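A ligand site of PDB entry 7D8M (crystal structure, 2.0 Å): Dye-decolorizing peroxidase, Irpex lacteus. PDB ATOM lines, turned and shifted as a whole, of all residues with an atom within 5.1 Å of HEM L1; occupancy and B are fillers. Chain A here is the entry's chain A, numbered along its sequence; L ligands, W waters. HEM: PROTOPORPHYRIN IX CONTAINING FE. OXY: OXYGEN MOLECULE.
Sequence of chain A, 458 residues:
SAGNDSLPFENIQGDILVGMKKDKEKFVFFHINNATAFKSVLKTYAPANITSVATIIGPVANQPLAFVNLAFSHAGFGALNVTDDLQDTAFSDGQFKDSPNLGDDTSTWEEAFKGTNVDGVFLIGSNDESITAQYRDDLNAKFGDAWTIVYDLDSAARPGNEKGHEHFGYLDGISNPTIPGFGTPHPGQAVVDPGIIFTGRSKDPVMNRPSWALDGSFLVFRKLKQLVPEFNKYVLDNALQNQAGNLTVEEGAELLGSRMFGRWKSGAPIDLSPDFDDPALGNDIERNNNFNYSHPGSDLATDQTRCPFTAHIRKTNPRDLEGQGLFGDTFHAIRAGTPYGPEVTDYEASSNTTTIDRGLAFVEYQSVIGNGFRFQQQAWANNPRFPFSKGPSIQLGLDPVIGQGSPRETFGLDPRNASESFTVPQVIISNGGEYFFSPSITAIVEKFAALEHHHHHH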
ATOM      1  N   GLU A 166      20.659 -31.434  -5.053  1.00  0.00           N
ATOM      2  CA  GLU A 166      20.562 -30.156  -5.728  1.00  0.00           C
ATOM      3  C   GLU A 166      20.147 -30.399  -7.185  1.00  0.00           C
ATOM      4  O   GLU A 166      20.045 -31.533  -7.646  1.00  0.00           O
ATOM      5  CB  GLU A 166      21.874 -29.370  -5.594  1.00  0.00           C
ATOM      6  CG  GLU A 166      23.131 -30.111  -6.049  1.00  0.00           C
ATOM      7  CD  GLU A 166      23.144 -30.293  -7.543  1.00  0.00           C
ATOM      8  OE1 GLU A 166      23.382 -31.421  -8.000  1.00  0.00           O
ATOM      9  OE2 GLU A 166      22.870 -29.301  -8.272  1.00  0.00           O
ATOM     10  N   PHE A 168      21.314 -30.206 -10.195  1.00  0.00           N
ATOM     11  CA  PHE A 168      22.030 -31.056 -11.139  1.00  0.00           C
ATOM     12  C   PHE A 168      21.813 -32.539 -10.852  1.00  0.00           C
ATOM     13  O   PHE A 168      22.167 -33.372 -11.692  1.00  0.00           O
ATOM     14  CB  PHE A 168      23.520 -30.747 -11.104  1.00  0.00           C
ATOM     15  CG  PHE A 168      23.896 -29.423 -11.713  1.00  0.00           C
ATOM     16  CD1 PHE A 168      23.384 -29.041 -12.942  1.00  0.00           C
ATOM     17  CD2 PHE A 168      24.773 -28.575 -11.066  1.00  0.00           C
ATOM     18  CE1 PHE A 168      23.737 -27.815 -13.502  1.00  0.00           C
ATOM     19  CE2 PHE A 168      25.126 -27.349 -11.626  1.00  0.00           C
ATOM     20  CZ  PHE A 168      24.615 -26.973 -12.848  1.00  0.00           C
ATOM     21  N   TYR A 170      22.733 -34.179  -7.727  1.00  0.00           N
ATOM     22  CA  TYR A 170      23.680 -34.768  -6.787  1.00  0.00           C
ATOM     23  C   TYR A 170      23.168 -34.592  -5.372  1.00  0.00           C
ATOM     24  O   TYR A 170      22.718 -33.503  -4.995  1.00  0.00           O
ATOM     25  CB  TYR A 170      25.059 -34.133  -6.941  1.00  0.00           C
ATOM     26  CG  TYR A 170      25.682 -34.528  -8.259  1.00  0.00           C
ATOM     27  CD1 TYR A 170      25.275 -33.924  -9.445  1.00  0.00           C
ATOM     28  CD2 TYR A 170      26.642 -35.532  -8.330  1.00  0.00           C
ATOM     29  CE1 TYR A 170      25.827 -34.299 -10.666  1.00  0.00           C
ATOM     30  CE2 TYR A 170      27.182 -35.926  -9.553  1.00  0.00           C
ATOM     31  CZ  TYR A 170      26.774 -35.308 -10.713  1.00  0.00           C
ATOM     32  OH  TYR A 170      27.297 -35.677 -11.924  1.00  0.00           O
ATOM     33  N   LEU A 171      23.218 -35.668  -4.585  1.00  0.00           N
ATOM     34  CA  LEU A 171      22.891 -35.560  -3.175  1.00  0.00           C
ATOM     35  C   LEU A 171      23.776 -34.514  -2.509  1.00  0.00           C
ATOM     36  O   LEU A 171      25.009 -34.505  -2.697  1.00  0.00           O
ATOM     37  CB  LEU A 171      23.054 -36.911  -2.480  1.00  0.00           C
ATOM     38  CG  LEU A 171      22.622 -36.933  -1.014  1.00  0.00           C
ATOM     39  CD1 LEU A 171      21.130 -36.592  -0.878  1.00  0.00           C
ATOM     40  CD2 LEU A 171      22.959 -38.270  -0.369  1.00  0.00           C
ATOM     41  N   ASP A 172      23.156 -33.614  -1.764  1.00  0.00           N
ATOM     42  CA  ASP A 172      23.838 -32.484  -1.174  1.00  0.00           C
ATOM     43  C   ASP A 172      23.653 -32.536   0.344  1.00  0.00           C
ATOM     44  O   ASP A 172      22.915 -33.368   0.866  1.00  0.00           O
ATOM     45  CB  ASP A 172      23.291 -31.167  -1.756  1.00  0.00           C
ATOM     46  CG  ASP A 172      24.273 -30.021  -1.629  1.00  0.00           C
ATOM     47  OD1 ASP A 172      25.223 -30.133  -0.820  1.00  0.00           O
ATOM     48  OD2 ASP A 172      24.075 -28.992  -2.318  1.00  0.00           O
ATOM     49  N   GLY A 173      24.333 -31.627   1.043  1.00  0.00           N
ATOM     50  CA  GLY A 173      24.252 -31.615   2.484  1.00  0.00           C
ATOM     51  C   GLY A 173      24.862 -32.833   3.151  1.00  0.00           C
ATOM     52  O   GLY A 173      24.378 -33.253   4.208  1.00  0.00           O
ATOM     53  N   ILE A 174      25.905 -33.402   2.568  1.00  0.00           N
ATOM     54  CA  ILE A 174      26.565 -34.569   3.166  1.00  0.00           C
ATOM     55  C   ILE A 174      27.639 -34.149   4.157  1.00  0.00           C
ATOM     56  O   ILE A 174      27.618 -34.559   5.317  1.00  0.00           O
ATOM     57  CB  ILE A 174      27.157 -35.488   2.078  1.00  0.00           C
ATOM     58  CG1 ILE A 174      26.055 -36.029   1.170  1.00  0.00           C
ATOM     59  CG2 ILE A 174      27.935 -36.620   2.721  1.00  0.00           C
ATOM     60  CD1 ILE A 174      26.565 -36.624  -0.143  1.00  0.00           C
ATOM     61  N   SER A 175      28.599 -33.318   3.729  1.00  0.00           N
ATOM     62  CA  SER A 175      29.786 -33.008   4.506  1.00  0.00           C
ATOM     63  C   SER A 175      29.717 -31.581   5.056  1.00  0.00           C
ATOM     64  O   SER A 175      29.743 -30.612   4.295  1.00  0.00           O
ATOM     65  CB  SER A 175      31.051 -33.187   3.656  1.00  0.00           C
ATOM     66  OG  SER A 175      32.212 -32.960   4.426  1.00  0.00           O
ATOM     67  N   LEU A 224      22.473 -18.670  -6.680  1.00  0.00           N
ATOM     68  CA  LEU A 224      23.286 -19.315  -7.718  1.00  0.00           C
ATOM     69  C   LEU A 224      22.372 -20.025  -8.698  1.00  0.00           C
ATOM     70  O   LEU A 224      21.863 -21.117  -8.407  1.00  0.00           O
ATOM     71  CB  LEU A 224      24.306 -20.254  -7.102  1.00  0.00           C
ATOM     72  CG  LEU A 224      25.261 -19.589  -6.101  1.00  0.00           C
ATOM     73  CD1 LEU A 224      26.189 -20.603  -5.475  1.00  0.00           C
ATOM     74  CD2 LEU A 224      26.053 -18.434  -6.741  1.00  0.00           C
ATOM     75  N   GLN A 226      21.262 -22.189 -11.888  1.00  0.00           N
ATOM     76  CA  GLN A 226      21.836 -23.410 -12.445  1.00  0.00           C
ATOM     77  C   GLN A 226      21.232 -23.721 -13.806  1.00  0.00           C
ATOM     78  O   GLN A 226      20.004 -23.715 -13.964  1.00  0.00           O
ATOM     79  CB  GLN A 226      21.625 -24.606 -11.504  1.00  0.00           C
ATOM     80  CG  GLN A 226      22.526 -24.582 -10.285  1.00  0.00           C
ATOM     81  CD  GLN A 226      22.190 -25.661  -9.273  1.00  0.00           C
ATOM     82  OE1 GLN A 226      21.545 -25.388  -8.260  1.00  0.00           O
ATOM     83  NE2 GLN A 226      22.630 -26.897  -9.538  1.00  0.00           N
ATOM     84  N   PHE A 261      32.410 -33.304  -9.633  1.00  0.00           N
ATOM     85  CA  PHE A 261      31.928 -33.015  -8.294  1.00  0.00           C
ATOM     86  C   PHE A 261      32.784 -33.658  -7.201  1.00  0.00           C
ATOM     87  O   PHE A 261      33.006 -33.042  -6.154  1.00  0.00           O
ATOM     88  CB  PHE A 261      30.473 -33.476  -8.145  1.00  0.00           C
ATOM     89  CG  PHE A 261      29.478 -32.479  -8.655  1.00  0.00           C
ATOM     90  CD1 PHE A 261      29.043 -31.438  -7.857  1.00  0.00           C
ATOM     91  CD2 PHE A 261      29.002 -32.576  -9.954  1.00  0.00           C
ATOM     92  CE1 PHE A 261      28.135 -30.503  -8.325  1.00  0.00           C
ATOM     93  CE2 PHE A 261      28.101 -31.649 -10.445  1.00  0.00           C
ATOM     94  CZ  PHE A 261      27.666 -30.604  -9.629  1.00  0.00           C
ATOM     95  N   ARG A 263      31.688 -36.752  -6.306  1.00  0.00           N
ATOM     96  CA  ARG A 263      30.676 -37.687  -5.845  1.00  0.00           C
ATOM     97  C   ARG A 263      29.798 -38.053  -7.030  1.00  0.00           C
ATOM     98  O   ARG A 263      29.617 -37.246  -7.957  1.00  0.00           O
ATOM     99  CB  ARG A 263      29.794 -37.114  -4.727  1.00  0.00           C
ATOM    100  CG  ARG A 263      30.513 -36.884  -3.403  1.00  0.00           C
ATOM    101  CD  ARG A 263      29.540 -36.397  -2.327  1.00  0.00           C
ATOM    102  NE  ARG A 263      30.236 -36.050  -1.097  1.00  0.00           N
ATOM    103  CZ  ARG A 263      30.509 -36.913  -0.123  1.00  0.00           C
ATOM    104  NH1 ARG A 263      30.116 -38.177  -0.227  1.00  0.00           N
ATOM    105  NH2 ARG A 263      31.161 -36.515   0.956  1.00  0.00           N
ATOM    106  N   ASN A 289      31.183 -40.270   3.983  1.00  0.00           N
ATOM    107  CA  ASN A 289      32.153 -39.196   4.195  1.00  0.00           C
ATOM    108  C   ASN A 289      33.479 -39.688   4.739  1.00  0.00           C
ATOM    109  O   ASN A 289      34.338 -38.868   5.084  1.00  0.00           O
ATOM    110  CB  ASN A 289      31.577 -38.126   5.136  1.00  0.00           C
ATOM    111  CG  ASN A 289      31.992 -36.726   4.718  1.00  0.00           C
ATOM    112  OD1 ASN A 289      32.359 -36.495   3.552  1.00  0.00           O
ATOM    113  ND2 ASN A 289      31.955 -35.780   5.653  1.00  0.00           N
ATOM    114  N   PHE A 291      36.647 -40.654   4.054  1.00  0.00           N
ATOM    115  CA  PHE A 291      37.711 -40.652   3.068  1.00  0.00           C
ATOM    116  C   PHE A 291      38.540 -39.389   3.242  1.00  0.00           C
ATOM    117  O   PHE A 291      38.067 -38.384   3.777  1.00  0.00           O
ATOM    118  CB  PHE A 291      37.167 -40.737   1.637  1.00  0.00           C
ATOM    119  CG  PHE A 291      36.311 -39.550   1.248  1.00  0.00           C
ATOM    120  CD1 PHE A 291      36.862 -38.478   0.560  1.00  0.00           C
ATOM    121  CD2 PHE A 291      34.949 -39.522   1.528  1.00  0.00           C
ATOM    122  CE1 PHE A 291      36.074 -37.387   0.195  1.00  0.00           C
ATOM    123  CE2 PHE A 291      34.155 -38.444   1.166  1.00  0.00           C
ATOM    124  CZ  PHE A 291      34.714 -37.379   0.497  1.00  0.00           C
ATOM    125  N   TYR A 293      41.306 -38.984   0.575  1.00  0.00           N
ATOM    126  CA  TYR A 293      42.036 -39.037  -0.682  1.00  0.00           C
ATOM    127  C   TYR A 293      43.335 -39.843  -0.582  1.00  0.00           C
ATOM    128  O   TYR A 293      43.968 -40.074  -1.609  1.00  0.00           O
ATOM    129  CB  TYR A 293      42.306 -37.639  -1.235  1.00  0.00           C
ATOM    130  CG  TYR A 293      41.022 -36.849  -1.379  1.00  0.00           C
ATOM    131  CD1 TYR A 293      40.029 -37.266  -2.253  1.00  0.00           C
ATOM    132  CD2 TYR A 293      40.784 -35.719  -0.604  1.00  0.00           C
ATOM    133  CE1 TYR A 293      38.833 -36.558  -2.375  1.00  0.00           C
ATOM    134  CE2 TYR A 293      39.587 -35.001  -0.717  1.00  0.00           C
ATOM    135  CZ  TYR A 293      38.616 -35.431  -1.605  1.00  0.00           C
ATOM    136  OH  TYR A 293      37.429 -34.748  -1.752  1.00  0.00           O
ATOM    137  N   HIS A 312      35.191 -30.599  -7.315  1.00  0.00           N
ATOM    138  CA  HIS A 312      34.577 -29.548  -6.512  1.00  0.00           C
ATOM    139  C   HIS A 312      34.839 -29.735  -5.026  1.00  0.00           C
ATOM    140  O   HIS A 312      35.377 -28.835  -4.372  1.00  0.00           O
ATOM    141  CB  HIS A 312      33.067 -29.525  -6.784  1.00  0.00           C
ATOM    142  CG  HIS A 312      32.343 -28.503  -5.981  1.00  0.00           C
ATOM    143  ND1 HIS A 312      32.804 -27.208  -5.842  1.00  0.00           N
ATOM    144  CD2 HIS A 312      31.208 -28.574  -5.257  1.00  0.00           C
ATOM    145  CE1 HIS A 312      31.974 -26.532  -5.075  1.00  0.00           C
ATOM    146  NE2 HIS A 312      30.988 -27.333  -4.711  1.00  0.00           N
ATOM    147  N   ILE A 313      34.509 -30.904  -4.484  1.00  0.00           N
ATOM    148  CA  ILE A 313      34.636 -31.101  -3.032  1.00  0.00           C
ATOM    149  C   ILE A 313      36.094 -31.133  -2.611  1.00  0.00           C
ATOM    150  O   ILE A 313      36.426 -30.799  -1.471  1.00  0.00           O
ATOM    151  CB  ILE A 313      33.895 -32.367  -2.558  1.00  0.00           C
ATOM    152  CG1 ILE A 313      34.561 -33.643  -3.069  1.00  0.00           C
ATOM    153  CG2 ILE A 313      32.413 -32.298  -2.928  1.00  0.00           C
ATOM    154  CD1 ILE A 313      34.086 -34.882  -2.341  1.00  0.00           C
ATOM    155  N   THR A 316      37.188 -27.336  -2.487  1.00  0.00           N
ATOM    156  CA  THR A 316      36.624 -26.545  -1.384  1.00  0.00           C
ATOM    157  C   THR A 316      36.919 -27.124  -0.008  1.00  0.00           C
ATOM    158  O   THR A 316      36.768 -26.429   0.995  1.00  0.00           O
ATOM    159  CB  THR A 316      35.111 -26.401  -1.528  1.00  0.00           C
ATOM    160  OG1 THR A 316      34.520 -27.712  -1.528  1.00  0.00           O
ATOM    161  CG2 THR A 316      34.767 -25.671  -2.810  1.00  0.00           C
ATOM    162  N   ASN A 317      37.308 -28.402   0.065  1.00  0.00           N
ATOM    163  CA  ASN A 317      37.781 -29.018   1.301  1.00  0.00           C
ATOM    164  C   ASN A 317      38.930 -29.933   0.917  1.00  0.00           C
ATOM    165  O   ASN A 317      38.748 -31.134   0.693  1.00  0.00           O
ATOM    166  CB  ASN A 317      36.671 -29.785   2.028  1.00  0.00           C
ATOM    167  CG  ASN A 317      37.161 -30.480   3.298  1.00  0.00           C
ATOM    168  OD1 ASN A 317      38.329 -30.343   3.680  1.00  0.00           O
ATOM    169  ND2 ASN A 317      36.274 -31.219   3.955  1.00  0.00           N
ATOM    170  N   ARG A 319      41.049 -32.071   1.936  1.00  0.00           N
ATOM    171  CA  ARG A 319      41.300 -32.880   3.129  1.00  0.00           C
ATOM    172  C   ARG A 319      42.741 -33.375   3.172  1.00  0.00           C
ATOM    173  O   ARG A 319      43.310 -33.520   4.260  1.00  0.00           O
ATOM    174  CB  ARG A 319      40.333 -34.071   3.164  1.00  0.00           C
ATOM    175  CG  ARG A 319      38.863 -33.713   3.078  1.00  0.00           C
ATOM    176  CD  ARG A 319      38.002 -34.946   2.868  1.00  0.00           C
ATOM    177  NE  ARG A 319      36.606 -34.571   2.720  1.00  0.00           N
ATOM    178  CZ  ARG A 319      35.573 -35.335   3.082  1.00  0.00           C
ATOM    179  NH1 ARG A 319      35.786 -36.528   3.615  1.00  0.00           N
ATOM    180  NH2 ARG A 319      34.333 -34.887   2.900  1.00  0.00           N
ATOM    181  N   ARG A 335      27.390 -25.247   5.319  1.00  0.00           N
ATOM    182  CA  ARG A 335      26.429 -24.882   4.294  1.00  0.00           C
ATOM    183  C   ARG A 335      25.023 -25.264   4.745  1.00  0.00           C
ATOM    184  O   ARG A 335      24.804 -26.347   5.299  1.00  0.00           O
ATOM    185  CB  ARG A 335      26.777 -25.568   2.959  1.00  0.00           C
ATOM    186  CG  ARG A 335      28.117 -25.130   2.361  1.00  0.00           C
ATOM    187  CD  ARG A 335      28.630 -26.099   1.277  1.00  0.00           C
ATOM    188  NE  ARG A 335      28.829 -27.434   1.816  1.00  0.00           N
ATOM    189  CZ  ARG A 335      28.231 -28.521   1.352  1.00  0.00           C
ATOM    190  NH1 ARG A 335      27.398 -28.411   0.319  1.00  0.00           N
ATOM    191  NH2 ARG A 335      28.435 -29.695   1.918  1.00  0.00           N
ATOM    192  N   LEU A 360      20.325 -22.738  -6.582  1.00  0.00           N
ATOM    193  CA  LEU A 360      20.605 -22.982  -5.179  1.00  0.00           C
ATOM    194  C   LEU A 360      20.551 -21.662  -4.455  1.00  0.00           C
ATOM    195  O   LEU A 360      21.266 -20.718  -4.829  1.00  0.00           O
ATOM    196  CB  LEU A 360      21.977 -23.656  -5.005  1.00  0.00           C
ATOM    197  CG  LEU A 360      22.430 -23.980  -3.575  1.00  0.00           C
ATOM    198  CD1 LEU A 360      21.447 -24.941  -2.909  1.00  0.00           C
ATOM    199  CD2 LEU A 360      23.836 -24.558  -3.592  1.00  0.00           C
ATOM    200  N   PHE A 362      22.074 -20.414  -1.806  1.00  0.00           N
ATOM    201  CA  PHE A 362      23.256 -20.863  -1.094  1.00  0.00           C
ATOM    202  C   PHE A 362      23.464 -20.065   0.194  1.00  0.00           C
ATOM    203  O   PHE A 362      23.452 -18.833   0.182  1.00  0.00           O
ATOM    204  CB  PHE A 362      24.472 -20.736  -2.023  1.00  0.00           C
ATOM    205  CG  PHE A 362      25.784 -21.088  -1.402  1.00  0.00           C
ATOM    206  CD1 PHE A 362      26.305 -22.377  -1.521  1.00  0.00           C
ATOM    207  CD2 PHE A 362      26.548 -20.114  -0.775  1.00  0.00           C
ATOM    208  CE1 PHE A 362      27.533 -22.698  -0.971  1.00  0.00           C
ATOM    209  CE2 PHE A 362      27.783 -20.432  -0.237  1.00  0.00           C
ATOM    210  CZ  PHE A 362      28.277 -21.734  -0.324  1.00  0.00           C
ATOM    211  N   GLU A 364      26.142 -20.113   3.672  1.00  0.00           N
ATOM    212  CA  GLU A 364      27.314 -20.682   4.313  1.00  0.00           C
ATOM    213  C   GLU A 364      27.681 -19.852   5.530  1.00  0.00           C
ATOM    214  O   GLU A 364      27.745 -18.620   5.453  1.00  0.00           O
ATOM    215  CB  GLU A 364      28.508 -20.751   3.341  1.00  0.00           C
ATOM    216  CG  GLU A 364      29.651 -21.609   3.852  1.00  0.00           C
ATOM    217  CD  GLU A 364      30.680 -21.956   2.777  1.00  0.00           C
ATOM    218  OE1 GLU A 364      30.844 -21.173   1.825  1.00  0.00           O
ATOM    219  OE2 GLU A 364      31.298 -23.038   2.882  1.00  0.00           O
ATOM    220  N   PHE A 373      33.619 -19.201   3.041  1.00  0.00           N
ATOM    221  CA  PHE A 373      33.098 -19.019   1.693  1.00  0.00           C
ATOM    222  C   PHE A 373      34.112 -18.335   0.776  1.00  0.00           C
ATOM    223  O   PHE A 373      34.400 -18.813  -0.330  1.00  0.00           O
ATOM    224  CB  PHE A 373      31.820 -18.182   1.716  1.00  0.00           C
ATOM    225  CG  PHE A 373      31.514 -17.548   0.394  1.00  0.00           C
ATOM    226  CD1 PHE A 373      30.966 -18.306  -0.636  1.00  0.00           C
ATOM    227  CD2 PHE A 373      31.827 -16.215   0.161  1.00  0.00           C
ATOM    228  CE1 PHE A 373      30.718 -17.726  -1.865  1.00  0.00           C
ATOM    229  CE2 PHE A 373      31.573 -15.647  -1.066  1.00  0.00           C
ATOM    230  CZ  PHE A 373      31.017 -16.391  -2.081  1.00  0.00           C
ATOM    231  N   GLN A 376      37.242 -20.426  -0.024  1.00  0.00           N
ATOM    232  CA  GLN A 376      36.854 -21.561  -0.849  1.00  0.00           C
ATOM    233  C   GLN A 376      36.581 -21.130  -2.284  1.00  0.00           C
ATOM    234  O   GLN A 376      36.987 -21.812  -3.237  1.00  0.00           O
ATOM    235  CB  GLN A 376      35.619 -22.241  -0.245  1.00  0.00           C
ATOM    236  CG  GLN A 376      35.861 -22.937   1.096  1.00  0.00           C
ATOM    237  CD  GLN A 376      34.558 -23.228   1.840  1.00  0.00           C
ATOM    238  OE1 GLN A 376      33.476 -23.151   1.262  1.00  0.00           O
ATOM    239  NE2 GLN A 376      34.659 -23.549   3.124  1.00  0.00           N
ATOM    240  N   GLN A 377      35.933 -19.976  -2.455  1.00  0.00           N
ATOM    241  CA  GLN A 377      35.648 -19.472  -3.793  1.00  0.00           C
ATOM    242  C   GLN A 377      36.900 -18.899  -4.458  1.00  0.00           C
ATOM    243  O   GLN A 377      37.309 -19.360  -5.521  1.00  0.00           O
ATOM    244  CB  GLN A 377      34.526 -18.421  -3.725  1.00  0.00           C
ATOM    245  CG  GLN A 377      34.090 -17.917  -5.085  1.00  0.00           C
ATOM    246  CD  GLN A 377      33.302 -18.959  -5.869  1.00  0.00           C
ATOM    247  OE1 GLN A 377      32.191 -19.330  -5.486  1.00  0.00           O
ATOM    248  NE2 GLN A 377      33.880 -19.426  -6.972  1.00  0.00           N
ATOM    249  N   VAL A 401      32.800 -26.856 -11.283  1.00  0.00           N
ATOM    250  CA  VAL A 401      31.427 -26.573 -10.901  1.00  0.00           C
ATOM    251  C   VAL A 401      31.285 -25.075 -10.660  1.00  0.00           C
ATOM    252  O   VAL A 401      30.595 -24.381 -11.410  1.00  0.00           O
ATOM    253  CB  VAL A 401      31.006 -27.415  -9.683  1.00  0.00           C
ATOM    254  CG1 VAL A 401      29.537 -27.150  -9.250  1.00  0.00           C
ATOM    255  CG2 VAL A 401      31.194 -28.900  -9.985  1.00  0.00           C
ATOM    256  N   ILE A 402      31.999 -24.546  -9.661  1.00  0.00           N
ATOM    257  CA  ILE A 402      31.810 -23.162  -9.232  1.00  0.00           C
ATOM    258  C   ILE A 402      32.938 -22.232  -9.657  1.00  0.00           C
ATOM    259  O   ILE A 402      32.834 -21.018  -9.412  1.00  0.00           O
ATOM    260  CB  ILE A 402      31.609 -23.070  -7.701  1.00  0.00           C
ATOM    261  CG1 ILE A 402      32.850 -23.597  -6.974  1.00  0.00           C
ATOM    262  CG2 ILE A 402      30.331 -23.795  -7.299  1.00  0.00           C
ATOM    263  CD1 ILE A 402      32.987 -23.089  -5.521  1.00  0.00           C
ATOM    264  N   ILE A 428      26.726 -22.519 -13.654  1.00  0.00           N
ATOM    265  CA  ILE A 428      26.255 -21.838 -12.459  1.00  0.00           C
ATOM    266  C   ILE A 428      26.525 -20.361 -12.662  1.00  0.00           C
ATOM    267  O   ILE A 428      27.656 -19.966 -12.956  1.00  0.00           O
ATOM    268  CB  ILE A 428      26.968 -22.368 -11.200  1.00  0.00           C
ATOM    269  CG1 ILE A 428      26.532 -23.803 -10.922  1.00  0.00           C
ATOM    270  CG2 ILE A 428      26.693 -21.467 -10.002  1.00  0.00           C
ATOM    271  CD1 ILE A 428      27.341 -24.470  -9.860  1.00  0.00           C
HETATM  272  CHA HEM L   1      30.005 -29.896  -1.444  1.00  0.00           C
HETATM  273  CHB HEM L   1      27.093 -28.783  -5.159  1.00  0.00           C
HETATM  274  CHC HEM L   1      28.167 -24.090  -4.549  1.00  0.00           C
HETATM  275  CHD HEM L   1      31.447 -25.263  -1.171  1.00  0.00           C
HETATM  276  C1A HEM L   1      29.104 -30.016  -2.477  1.00  0.00           C
HETATM  277  C2A HEM L   1      28.457 -31.234  -2.920  1.00  0.00           C
HETATM  278  C3A HEM L   1      27.644 -30.919  -3.942  1.00  0.00           C
HETATM  279  C4A HEM L   1      27.755 -29.495  -4.175  1.00  0.00           C
HETATM  280  CMA HEM L   1      26.737 -31.858  -4.752  1.00  0.00           C
HETATM  281  CAA HEM L   1      28.687 -32.634  -2.280  1.00  0.00           C
HETATM  282  CBA HEM L   1      27.707 -32.861  -1.131  1.00  0.00           C
HETATM  283  CGA HEM L   1      28.371 -32.641   0.219  1.00  0.00           C
HETATM  284  O1A HEM L   1      29.564 -32.989   0.363  1.00  0.00           O
HETATM  285  O2A HEM L   1      27.691 -32.132   1.155  1.00  0.00           O
HETATM  286  C1B HEM L   1      27.107 -27.420  -5.285  1.00  0.00           C
HETATM  287  C2B HEM L   1      26.278 -26.665  -6.195  1.00  0.00           C
HETATM  288  C3B HEM L   1      26.589 -25.361  -6.028  1.00  0.00           C
HETATM  289  C4B HEM L   1      27.606 -25.262  -5.002  1.00  0.00           C
HETATM  290  CMB HEM L   1      25.264 -27.315  -7.175  1.00  0.00           C
HETATM  291  CAB HEM L   1      25.990 -24.114  -6.724  1.00  0.00           C
HETATM  292  CBB HEM L   1      24.801 -24.108  -7.341  1.00  0.00           C
HETATM  293  C1C HEM L   1      29.202 -23.991  -3.635  1.00  0.00           C
HETATM  294  C2C HEM L   1      29.934 -22.782  -3.279  1.00  0.00           C
HETATM  295  C3C HEM L   1      30.838 -23.106  -2.333  1.00  0.00           C
HETATM  296  C4C HEM L   1      30.721 -24.532  -2.087  1.00  0.00           C
HETATM  297  CMC HEM L   1      29.635 -21.393  -3.894  1.00  0.00           C
HETATM  298  CAC HEM L   1      31.891 -22.220  -1.618  1.00  0.00           C
HETATM  299  CBC HEM L   1      32.367 -21.074  -2.144  1.00  0.00           C
HETATM  300  C1D HEM L   1      31.250 -26.594  -0.867  1.00  0.00           C
HETATM  301  C2D HEM L   1      31.803 -27.316   0.260  1.00  0.00           C
HETATM  302  C3D HEM L   1      31.412 -28.589   0.187  1.00  0.00           C
HETATM  303  C4D HEM L   1      30.586 -28.720  -1.004  1.00  0.00           C
HETATM  304  CMD HEM L   1      32.707 -26.748   1.368  1.00  0.00           C
HETATM  305  CAD HEM L   1      31.778 -29.720   1.173  1.00  0.00           C
HETATM  306  CBD HEM L   1      33.088 -30.361   0.710  1.00  0.00           C
HETATM  307  CGD HEM L   1      33.580 -31.407   1.690  1.00  0.00           C
HETATM  308  O1D HEM L   1      34.067 -32.468   1.225  1.00  0.00           O
HETATM  309  O2D HEM L   1      33.465 -31.193   2.925  1.00  0.00           O
HETATM  310  NA  HEM L   1      28.661 -28.986  -3.272  1.00  0.00           N
HETATM  311  NB  HEM L   1      27.911 -26.541  -4.575  1.00  0.00           N
HETATM  312  NC  HEM L   1      29.716 -25.025  -2.893  1.00  0.00           N
HETATM  313  ND  HEM L   1      30.495 -27.479  -1.618  1.00  0.00           N
HETATM  314 FE   HEM L   1      29.310 -27.003  -3.213  1.00  0.00          FE
HETATM  315  O1  OXY L   2      25.189 -26.175  -0.720  1.00  0.00           O
HETATM  316  O2  OXY L   2      25.678 -26.817  -1.646  1.00  0.00           O
HETATM  317  O   HOH W   1      32.811 -29.115   4.547  1.00  0.00           O
HETATM  318  O   HOH W   2      36.735 -33.002   0.319  1.00  0.00           O
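An iron atom (FE) of HEM L1 is bound by a ring nitrogen (NE2) of His 312 (2.3 Å).
The backbone NH (N) of Ile 174 lies within hydrogen-bond range of an oxygen (O2A) of HEM L1, at 2.6 Å.
The backbone NH (N) of Ser 175 is in hydrogen-bond range of an oxygen (O2A) of HEM L1 (3.0 Å).
OG of Ser 175 sits at hydrogen-bond distance from O2D of HEM L1, 2.6 Å away.
NH2 of Arg 335 lies within salt-bridge range of O2A of HEM L1, at 2.7 Å.
O1D of HEM L1 is in salt-bridge range of NH2 of Arg 319 (3.0 Å).
ND2 of Asn 317 lies within hydrogen-bond range of O2D of HEM L1.
An oxygen (O2A) of HEM L1 lies within hydrogen-bond range of the backbone NH (N) of Gly 173, at 3.4 Å.
NE of Arg 263 lies within salt-bridge range of O1A of HEM L1, 3.5 Å away.
NH1 of Arg 335 is in hydrogen-bond range of O2 of OXY L2 (3.1 Å).
Residues that only touch HEM L1: Glu 166 (3.3 Å), Tyr 170 (3.6 Å), Leu 171 (3.5 Å), Asp 172 (3.7 Å), Leu 224 (3.7 Å), Gln 226 (3.6 Å), Phe 261 (3.8 Å), Ile 313 (3.7 Å), Thr 316 (3.3 Å), Leu 360 (3.7 Å), Phe 362 (3.3 Å), Glu 364 (3.7 Å), Phe 373 (3.4 Å), Gln 376 (3.4 Å), Gln 377 (3.7 Å), Ile 402 (3.5 Å) and Ile 428 (3.4 Å).
Of the 30 residues printed, 25 come within 4 Å of HEM L1.
The backbone carbonyl oxygen (O) of His 312 sits at hydrogen-bond distance from the side-chain hydroxyl (OG1) of Thr 316 (3.2 Å).
OG of Ser 175 is in hydrogen-bond range of NH2 of Arg 319, 3.2 Å away.
The side-chain amide nitrogen of Asn 289 is in hydrogen-bond range of the side-chain hydroxyl of Ser 175, at 3.1 Å.
The side-chain amide oxygen (OD1) of Asn 289 sits at hydrogen-bond distance from the guanidinium group (NH2) of Arg 319 (2.6 Å).
OD1 of Asn 289 lies within hydrogen-bond range of NH2 of Arg 263, 2.9 Å away.
The backbone carbonyl oxygen (O) of Ile 402 lies within hydrogen-bond range of the side-chain amide nitrogen (NE2) of Gln 377 (3.1 Å).
The backbone NH (N) of Leu 360 is in hydrogen-bond range of the backbone carbonyl oxygen (O) of Leu 224 (2.9 Å).
The backbone carbonyl oxygen (O) of Phe 261 is in hydrogen-bond range of the backbone NH (N) of Ile 313, 3.1 Å away.
Water W1 lies within hydrogen-bond range of O2D of HEM L1 and O of Ser 175.
Water W2 lies within hydrogen-bond range of O of Asn 317 (2.8 Å), OH of Tyr 293 (2.8 Å), O of Ile 313 (2.9 Å), O1D of HEM L1 (2.9 Å) and NE of Arg 319 (2.9 Å).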
